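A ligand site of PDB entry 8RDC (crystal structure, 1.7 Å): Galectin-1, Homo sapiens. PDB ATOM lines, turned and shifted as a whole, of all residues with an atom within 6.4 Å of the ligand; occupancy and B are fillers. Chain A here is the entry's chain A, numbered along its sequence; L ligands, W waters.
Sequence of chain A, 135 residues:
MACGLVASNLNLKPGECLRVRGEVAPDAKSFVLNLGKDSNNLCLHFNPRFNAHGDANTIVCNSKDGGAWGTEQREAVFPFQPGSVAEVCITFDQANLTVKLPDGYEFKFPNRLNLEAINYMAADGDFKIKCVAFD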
ATOM      1  N   SER A  30       9.228 -11.807 -26.542  1.00  0.00           N
ATOM      2  CA  SER A  30       9.775 -12.992 -27.243  1.00  0.00           C
ATOM      3  C   SER A  30       8.686 -13.586 -28.122  1.00  0.00           C
ATOM      4  O   SER A  30       7.498 -13.336 -27.867  1.00  0.00           O
ATOM      5  CB  SER A  30      10.337 -14.036 -26.304  1.00  0.00           C
ATOM      6  OG  SER A  30       9.292 -14.574 -25.503  1.00  0.00           O
ATOM      7  N   PHE A  31       9.084 -14.421 -29.065  1.00  0.00           N
ATOM      8  CA  PHE A  31       8.102 -15.229 -29.812  1.00  0.00           C
ATOM      9  C   PHE A  31       8.731 -16.542 -30.213  1.00  0.00           C
ATOM     10  O   PHE A  31       9.947 -16.709 -30.065  1.00  0.00           O
ATOM     11  CB  PHE A  31       7.486 -14.479 -31.003  1.00  0.00           C
ATOM     12  CG  PHE A  31       8.352 -14.278 -32.217  1.00  0.00           C
ATOM     13  CD1 PHE A  31       8.368 -15.237 -33.213  1.00  0.00           C
ATOM     14  CD2 PHE A  31       9.043 -13.093 -32.415  1.00  0.00           C
ATOM     15  CE1 PHE A  31       9.067 -15.024 -34.392  1.00  0.00           C
ATOM     16  CE2 PHE A  31       9.776 -12.893 -33.573  1.00  0.00           C
ATOM     17  CZ  PHE A  31       9.764 -13.856 -34.557  1.00  0.00           C
ATOM     18  N   VAL A  32       7.890 -17.472 -30.652  1.00  0.00           N
ATOM     19  CA  VAL A  32       8.329 -18.853 -30.920  1.00  0.00           C
ATOM     20  C   VAL A  32       7.717 -19.321 -32.234  1.00  0.00           C
ATOM     21  O   VAL A  32       6.503 -19.112 -32.460  1.00  0.00           O
ATOM     22  CB  VAL A  32       7.886 -19.794 -29.784  1.00  0.00           C
ATOM     23  CG1 VAL A  32       8.096 -21.242 -30.139  1.00  0.00           C
ATOM     24  CG2 VAL A  32       8.546 -19.454 -28.464  1.00  0.00           C
ATOM     25  N   HIS A  45      12.926 -25.429 -32.406  1.00  0.00           N
ATOM     26  CA  HIS A  45      12.265 -24.405 -31.582  1.00  0.00           C
ATOM     27  C   HIS A  45      13.037 -23.126 -31.879  1.00  0.00           C
ATOM     28  O   HIS A  45      14.230 -23.051 -31.521  1.00  0.00           O
ATOM     29  CB  HIS A  45      12.318 -24.832 -30.098  1.00  0.00           C
ATOM     30  CG  HIS A  45      11.916 -23.770 -29.117  1.00  0.00           C
ATOM     31  ND1 HIS A  45      10.618 -23.490 -28.863  1.00  0.00           N
ATOM     32  CD2 HIS A  45      12.653 -22.978 -28.309  1.00  0.00           C
ATOM     33  CE1 HIS A  45      10.537 -22.546 -27.922  1.00  0.00           C
ATOM     34  NE2 HIS A  45      11.801 -22.205 -27.561  1.00  0.00           N
ATOM     35  N   ASN A  47      13.309 -19.228 -31.301  1.00  0.00           N
ATOM     36  CA  ASN A  47      12.866 -18.375 -30.167  1.00  0.00           C
ATOM     37  C   ASN A  47      13.625 -17.048 -30.132  1.00  0.00           C
ATOM     38  O   ASN A  47      14.533 -16.857 -29.300  1.00  0.00           O
ATOM     39  CB  ASN A  47      12.947 -19.182 -28.862  1.00  0.00           C
ATOM     40  CG  ASN A  47      12.481 -18.465 -27.615  1.00  0.00           C
ATOM     41  OD1 ASN A  47      13.016 -18.753 -26.534  1.00  0.00           O
ATOM     42  ND2 ASN A  47      11.537 -17.550 -27.746  1.00  0.00           N
ATOM     43  N   ARG A  49      14.350 -13.654 -28.697  1.00  0.00           N
ATOM     44  CA  ARG A  49      14.150 -13.062 -27.358  1.00  0.00           C
ATOM     45  C   ARG A  49      14.560 -11.585 -27.418  1.00  0.00           C
ATOM     46  O   ARG A  49      15.756 -11.287 -27.523  1.00  0.00           O
ATOM     47  CB  ARG A  49      14.950 -13.840 -26.328  1.00  0.00           C
ATOM     48  CG  ARG A  49      14.513 -15.299 -26.190  1.00  0.00           C
ATOM     49  CD  ARG A  49      15.430 -16.098 -25.262  1.00  0.00           C
ATOM     50  NE  ARG A  49      15.004 -17.480 -25.168  1.00  0.00           N
ATOM     51  CZ  ARG A  49      15.494 -18.398 -24.332  1.00  0.00           C
ATOM     52  NH1 ARG A  49      16.468 -18.098 -23.474  1.00  0.00           N
ATOM     53  NH2 ARG A  49      15.013 -19.640 -24.346  1.00  0.00           N
ATOM     54  N   HIS A  53      13.952 -14.382 -20.371  1.00  0.00           N
ATOM     55  CA  HIS A  53      14.705 -15.558 -19.861  1.00  0.00           C
ATOM     56  C   HIS A  53      16.180 -15.174 -19.671  1.00  0.00           C
ATOM     57  O   HIS A  53      16.997 -16.072 -19.704  1.00  0.00           O
ATOM     58  CB  HIS A  53      14.539 -16.735 -20.819  1.00  0.00           C
ATOM     59  CG  HIS A  53      13.158 -16.937 -21.332  1.00  0.00           C
ATOM     60  ND1 HIS A  53      12.072 -16.990 -20.477  1.00  0.00           N
ATOM     61  CD2 HIS A  53      12.659 -17.102 -22.589  1.00  0.00           C
ATOM     62  CE1 HIS A  53      10.979 -17.215 -21.203  1.00  0.00           C
ATOM     63  NE2 HIS A  53      11.308 -17.263 -22.499  1.00  0.00           N
ATOM     64  N   VAL A  60      17.445 -17.689 -29.719  1.00  0.00           N
ATOM     65  CA  VAL A  60      17.774 -19.007 -29.124  1.00  0.00           C
ATOM     66  C   VAL A  60      17.050 -20.064 -29.945  1.00  0.00           C
ATOM     67  O   VAL A  60      15.832 -19.898 -30.199  1.00  0.00           O
ATOM     68  CB  VAL A  60      17.372 -19.084 -27.651  1.00  0.00           C
ATOM     69  CG1 VAL A  60      17.644 -20.490 -27.109  1.00  0.00           C
ATOM     70  CG2 VAL A  60      18.072 -17.996 -26.842  1.00  0.00           C
ATOM     71  N   CYS A  61      17.780 -21.065 -30.433  1.00  0.00           N
ATOM     72  CA  CYS A  61      17.170 -22.240 -31.095  1.00  0.00           C
ATOM     73  C   CYS A  61      17.493 -23.474 -30.256  1.00  0.00           C
ATOM     74  O   CYS A  61      18.573 -23.554 -29.600  1.00  0.00           O
ATOM     75  CB  CYS A  61      17.697 -22.456 -32.492  1.00  0.00           C
ATOM     76  SG  CYS A  61      17.151 -21.133 -33.610  1.00  0.00           S
ATOM     77  N   ASN A  62      16.585 -24.436 -30.304  1.00  0.00           N
ATOM     78  CA  ASN A  62      16.814 -25.736 -29.653  1.00  0.00           C
ATOM     79  C   ASN A  62      15.979 -26.788 -30.339  1.00  0.00           C
ATOM     80  O   ASN A  62      15.203 -26.458 -31.288  1.00  0.00           O
ATOM     81  CB  ASN A  62      16.475 -25.682 -28.146  1.00  0.00           C
ATOM     82  CG  ASN A  62      17.313 -26.631 -27.319  1.00  0.00           C
ATOM     83  OD1 ASN A  62      17.880 -27.601 -27.839  1.00  0.00           O
ATOM     84  ND2 ASN A  62      17.325 -26.381 -26.027  1.00  0.00           N
ATOM     85  N   SER A  63      16.231 -28.035 -29.969  1.00  0.00           N
ATOM     86  CA  SER A  63      15.416 -29.199 -30.337  1.00  0.00           C
ATOM     87  C   SER A  63      14.684 -29.698 -29.091  1.00  0.00           C
ATOM     88  O   SER A  63      15.088 -29.367 -27.960  1.00  0.00           O
ATOM     89  CB  SER A  63      16.273 -30.286 -30.936  1.00  0.00           C
ATOM     90  OG  SER A  63      17.289 -30.636 -30.004  1.00  0.00           O
ATOM     91  N   LYS A  64      13.710 -30.564 -29.286  1.00  0.00           N
ATOM     92  CA  LYS A  64      12.995 -31.219 -28.175  1.00  0.00           C
ATOM     93  C   LYS A  64      12.773 -32.662 -28.607  1.00  0.00           C
ATOM     94  O   LYS A  64      12.273 -32.865 -29.700  1.00  0.00           O
ATOM     95  CB  LYS A  64      11.671 -30.525 -27.872  1.00  0.00           C
ATOM     96  CG  LYS A  64      11.023 -31.013 -26.601  1.00  0.00           C
ATOM     97  CD  LYS A  64       9.742 -30.286 -26.209  1.00  0.00           C
ATOM     98  CE  LYS A  64      10.044 -29.232 -25.168  1.00  0.00           C
ATOM     99  NZ  LYS A  64       8.851 -28.773 -24.411  1.00  0.00           N
ATOM    100  N   TRP A  69      14.404 -30.890 -23.795  1.00  0.00           N
ATOM    101  CA  TRP A  69      15.213 -29.898 -24.547  1.00  0.00           C
ATOM    102  C   TRP A  69      16.612 -30.423 -24.847  1.00  0.00           C
ATOM    103  O   TRP A  69      17.261 -31.035 -23.928  1.00  0.00           O
ATOM    104  CB  TRP A  69      15.318 -28.569 -23.800  1.00  0.00           C
ATOM    105  CG  TRP A  69      14.026 -27.828 -23.651  1.00  0.00           C
ATOM    106  CD1 TRP A  69      13.387 -27.492 -22.477  1.00  0.00           C
ATOM    107  CD2 TRP A  69      13.254 -27.268 -24.719  1.00  0.00           C
ATOM    108  NE1 TRP A  69      12.246 -26.789 -22.772  1.00  0.00           N
ATOM    109  CE2 TRP A  69      12.146 -26.630 -24.127  1.00  0.00           C
ATOM    110  CE3 TRP A  69      13.387 -27.235 -26.110  1.00  0.00           C
ATOM    111  CZ2 TRP A  69      11.179 -25.975 -24.893  1.00  0.00           C
ATOM    112  CZ3 TRP A  69      12.434 -26.592 -26.867  1.00  0.00           C
ATOM    113  CH2 TRP A  69      11.321 -25.987 -26.266  1.00  0.00           C
ATOM    114  N   GLY A  70      17.110 -30.119 -26.037  1.00  0.00           N
ATOM    115  CA  GLY A  70      18.526 -30.336 -26.396  1.00  0.00           C
ATOM    116  C   GLY A  70      19.422 -29.211 -25.915  1.00  0.00           C
ATOM    117  O   GLY A  70      19.079 -28.521 -24.935  1.00  0.00           O
ATOM    118  N   THR A  71      20.593 -29.078 -26.533  1.00  0.00           N
ATOM    119  CA  THR A  71      21.515 -27.965 -26.230  1.00  0.00           C
ATOM    120  C   THR A  71      21.115 -26.706 -27.014  1.00  0.00           C
ATOM    121  O   THR A  71      20.909 -26.790 -28.234  1.00  0.00           O
ATOM    122  CB  THR A  71      22.975 -28.319 -26.526  1.00  0.00           C
ATOM    123  OG1 THR A  71      23.178 -29.626 -25.997  1.00  0.00           O
ATOM    124  CG2 THR A  71      23.931 -27.310 -25.934  1.00  0.00           C
ATOM    125  N   GLU A  72      21.062 -25.574 -26.321  1.00  0.00           N
ATOM    126  CA  GLU A  72      20.737 -24.284 -26.979  1.00  0.00           C
ATOM    127  C   GLU A  72      21.830 -23.836 -27.940  1.00  0.00           C
ATOM    128  O   GLU A  72      23.042 -24.082 -27.672  1.00  0.00           O
ATOM    129  CB  GLU A  72      20.461 -23.196 -25.927  1.00  0.00           C
ATOM    130  CG  GLU A  72      19.232 -23.498 -25.104  1.00  0.00           C
ATOM    131  CD  GLU A  72      18.948 -22.471 -24.013  1.00  0.00           C
ATOM    132  OE1 GLU A  72      19.932 -21.777 -23.581  1.00  0.00           O
ATOM    133  OE2 GLU A  72      17.776 -22.377 -23.573  1.00  0.00           O
ATOM    134  N   ASP A 124       3.845 -19.128 -31.152  1.00  0.00           N
ATOM    135  CA  ASP A 124       3.454 -18.671 -29.805  1.00  0.00           C
ATOM    136  C   ASP A 124       4.148 -17.341 -29.509  1.00  0.00           C
ATOM    137  O   ASP A 124       5.054 -16.949 -30.261  1.00  0.00           O
ATOM    138  CB  ASP A 124       3.755 -19.729 -28.758  1.00  0.00           C
ATOM    139  CG  ASP A 124       2.895 -19.684 -27.500  1.00  0.00           C
ATOM    140  OD1 ASP A 124       2.051 -18.778 -27.377  1.00  0.00           O
ATOM    141  OD2 ASP A 124       3.114 -20.568 -26.608  1.00  0.00           O
ATOM    142  N   GLY A 125       3.659 -16.637 -28.501  1.00  0.00           N
ATOM    143  CA  GLY A 125       4.314 -15.404 -28.039  1.00  0.00           C
ATOM    144  C   GLY A 125       3.914 -14.199 -28.870  1.00  0.00           C
ATOM    145  O   GLY A 125       2.807 -14.173 -29.473  1.00  0.00           O
ATOM    146  N   ASP A 126       4.806 -13.208 -28.911  1.00  0.00           N
ATOM    147  CA  ASP A 126       4.460 -11.798 -29.221  1.00  0.00           C
ATOM    148  C   ASP A 126       4.612 -11.539 -30.733  1.00  0.00           C
ATOM    149  O   ASP A 126       5.303 -10.595 -31.151  1.00  0.00           O
ATOM    150  CB  ASP A 126       5.295 -10.871 -28.334  1.00  0.00           C
ATOM    151  CG  ASP A 126       5.097 -11.098 -26.846  1.00  0.00           C
ATOM    152  OD1 ASP A 126       3.979 -11.500 -26.449  1.00  0.00           O
ATOM    153  OD2 ASP A 126       6.070 -10.949 -26.092  1.00  0.00           O
HETATM  154  C1  LIG L   1      10.044 -20.852 -23.969  1.00  0.00           C
HETATM  155  C2  LIG L   1       7.685 -20.031 -24.662  1.00  0.00           C
HETATM  156  C3  LIG L   1       8.697 -20.971 -24.171  1.00  0.00           C
HETATM  157  C4  LIG L   1      13.949 -22.116 -21.939  1.00  0.00           C
HETATM  158  C5  LIG L   1      12.543 -21.587 -22.237  1.00  0.00           C
HETATM  159  C6  LIG L   1      11.790 -22.517 -23.176  1.00  0.00           C
HETATM  160  C7  LIG L   1      13.965 -23.249 -24.085  1.00  0.00           C
HETATM  161  C8  LIG L   1      12.601 -22.696 -24.453  1.00  0.00           C
HETATM  162  C9  LIG L   1      14.874 -23.446 -25.266  1.00  0.00           C
HETATM  163  O1  LIG L   1      16.072 -24.102 -24.841  1.00  0.00           O
HETATM  164  O2  LIG L   1      14.650 -22.362 -23.170  1.00  0.00           O
HETATM  165  S1  LIG L   1      13.830 -23.607 -20.880  1.00  0.00           S
HETATM  166  N1  LIG L   1      10.430 -22.028 -23.442  1.00  0.00           N
HETATM  167  N2  LIG L   1       9.370 -22.851 -23.295  1.00  0.00           N
HETATM  168  N3  LIG L   1       8.317 -22.215 -23.755  1.00  0.00           N
HETATM  169  O3  LIG L   1      12.748 -21.459 -25.129  1.00  0.00           O
HETATM  170  O4  LIG L   1      11.764 -21.543 -21.047  1.00  0.00           O
HETATM  171  N4  LIG L   1       7.931 -18.814 -25.056  1.00  0.00           N
HETATM  172  C10 LIG L   1       6.777 -18.232 -25.486  1.00  0.00           C
HETATM  173  C11 LIG L   1       5.639 -18.972 -25.424  1.00  0.00           C
HETATM  174  S2  LIG L   1       6.018 -20.505 -24.787  1.00  0.00           S
HETATM  175  C12 LIG L   1      15.564 -23.989 -20.783  1.00  0.00           C
HETATM  176  C13 LIG L   1      16.474 -23.303 -19.923  1.00  0.00           C
HETATM  177  N5  LIG L   1      17.782 -23.598 -19.766  1.00  0.00           N
HETATM  178  C14 LIG L   1      18.278 -24.556 -20.554  1.00  0.00           C
HETATM  179  C15 LIG L   1      17.494 -25.256 -21.436  1.00  0.00           C
HETATM  180  C16 LIG L   1      16.138 -25.007 -21.543  1.00  0.00           C
HETATM  181 BR1  LIG L   1      18.285 -26.563 -22.562  1.00  0.00          BR
HETATM  182 CL1  LIG L   1       6.890 -16.631 -26.101  1.00  0.00          CL
HETATM  183  C17 LIG L   1      12.195 -20.567 -20.094  1.00  0.00           C
HETATM  184  C18 LIG L   1      15.996 -22.130 -19.228  1.00  0.00           C
HETATM  185  N6  LIG L   1      15.666 -21.181 -18.678  1.00  0.00           N
HETATM  186  O   HOH W   1      19.698 -22.067 -18.208  1.00  0.00           O
HETATM  187  O   HOH W   2      10.151 -17.163 -25.034  1.00  0.00           O
HETATM  188  O   HOH W   3      10.272 -25.247 -21.206  1.00  0.00           O
HETATM  189  O   HOH W   4      17.015 -20.393 -21.974  1.00  0.00           O
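The side-chain amide oxygen (OD1) of Asn 47 sits at hydrogen-bond distance from an oxygen (O3) of the ligand, 3.1 Å away.
A ring nitrogen (NE2) of His 45 sits at hydrogen-bond distance from an oxygen (O3) of the ligand, at 2.7 Å.
The side-chain carboxylate (OE2) of Glu 72 lies within hydrogen-bond range of an oxygen (O1) of the ligand (2.7 Å).
The guanidinium group (NH2) of Arg 49 is in hydrogen-bond range of an oxygen (O2) of the ligand.
O1 of the ligand sits at hydrogen-bond distance from ND2 of Asn 62 (2.9 Å).
The side-chain carboxylate (OD2) of Asp 124 lies close to a sulfur (S2) of the ligand (3.4 Å).
Ser 30 touches the ligand.
CG2 of Val 32 touches N4 of the ligand, at 3.5 Å.
His 53 touches the ligand.
Trp 69 touches the ligand.
O of Gly 70 touches BR1 of the ligand, 3.2 Å away.
Gly 125 touches the ligand.
Hydrophobic or aromatic side chains that line the ligand: Val 32, His 45, His 53 and Trp 69.
Within 4 Å of the ligand: Ser 30, Val 32, His 45, Asn 47, Arg 49, His 53, Asn 62, Trp 69, Gly 70, Glu 72, Asp 124 and Gly 125.
The nearest printed residue that does not touch the ligand is Phe 31 (4.1 Å).
Water W2 lies within hydrogen-bond range of N4 of the ligand, OG of Ser 30, NE2 of His 53 and ND2 of Asn 47.
Water W4 lies within hydrogen-bond range of OE2 of Glu 72 (2.7 Å), NH1 of Arg 49 (2.8 Å) and O2 of the ligand (3.3 Å).
Water W3 lies within hydrogen-bond range of the indole nitrogen (NE1) of Trp 69 (3.0 Å) and a nitrogen (N2) of the ligand (3.3 Å).
The side-chain amide nitrogen (ND2) of Asn 47 sits at hydrogen-bond distance from the backbone carbonyl oxygen (O) of Phe 31, at 2.9 Å.
The backbone carbonyl oxygen of Gly 70 is in hydrogen-bond range of the side-chain amide nitrogen of Asn 62 (3.0 Å).
The backbone NH of Gly 70 lies within hydrogen-bond range of the backbone carbonyl oxygen of Ser 63 (2.9 Å).
O of Asp 124 is in hydrogen-bond range of N of Val 32 (2.9 Å).
The backbone NH (N) of Asn 47 lies within hydrogen-bond range of the backbone carbonyl oxygen (O) of Val 60 (2.8 Å).
O of Thr 71 lies close to OD1 of Asn 62.
OE2 of Glu 72 is in salt-bridge range of NH2 of Arg 49, 3.97 Å away.
The backbone NH of His 45 lies within hydrogen-bond range of the backbone carbonyl oxygen of Asn 62.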
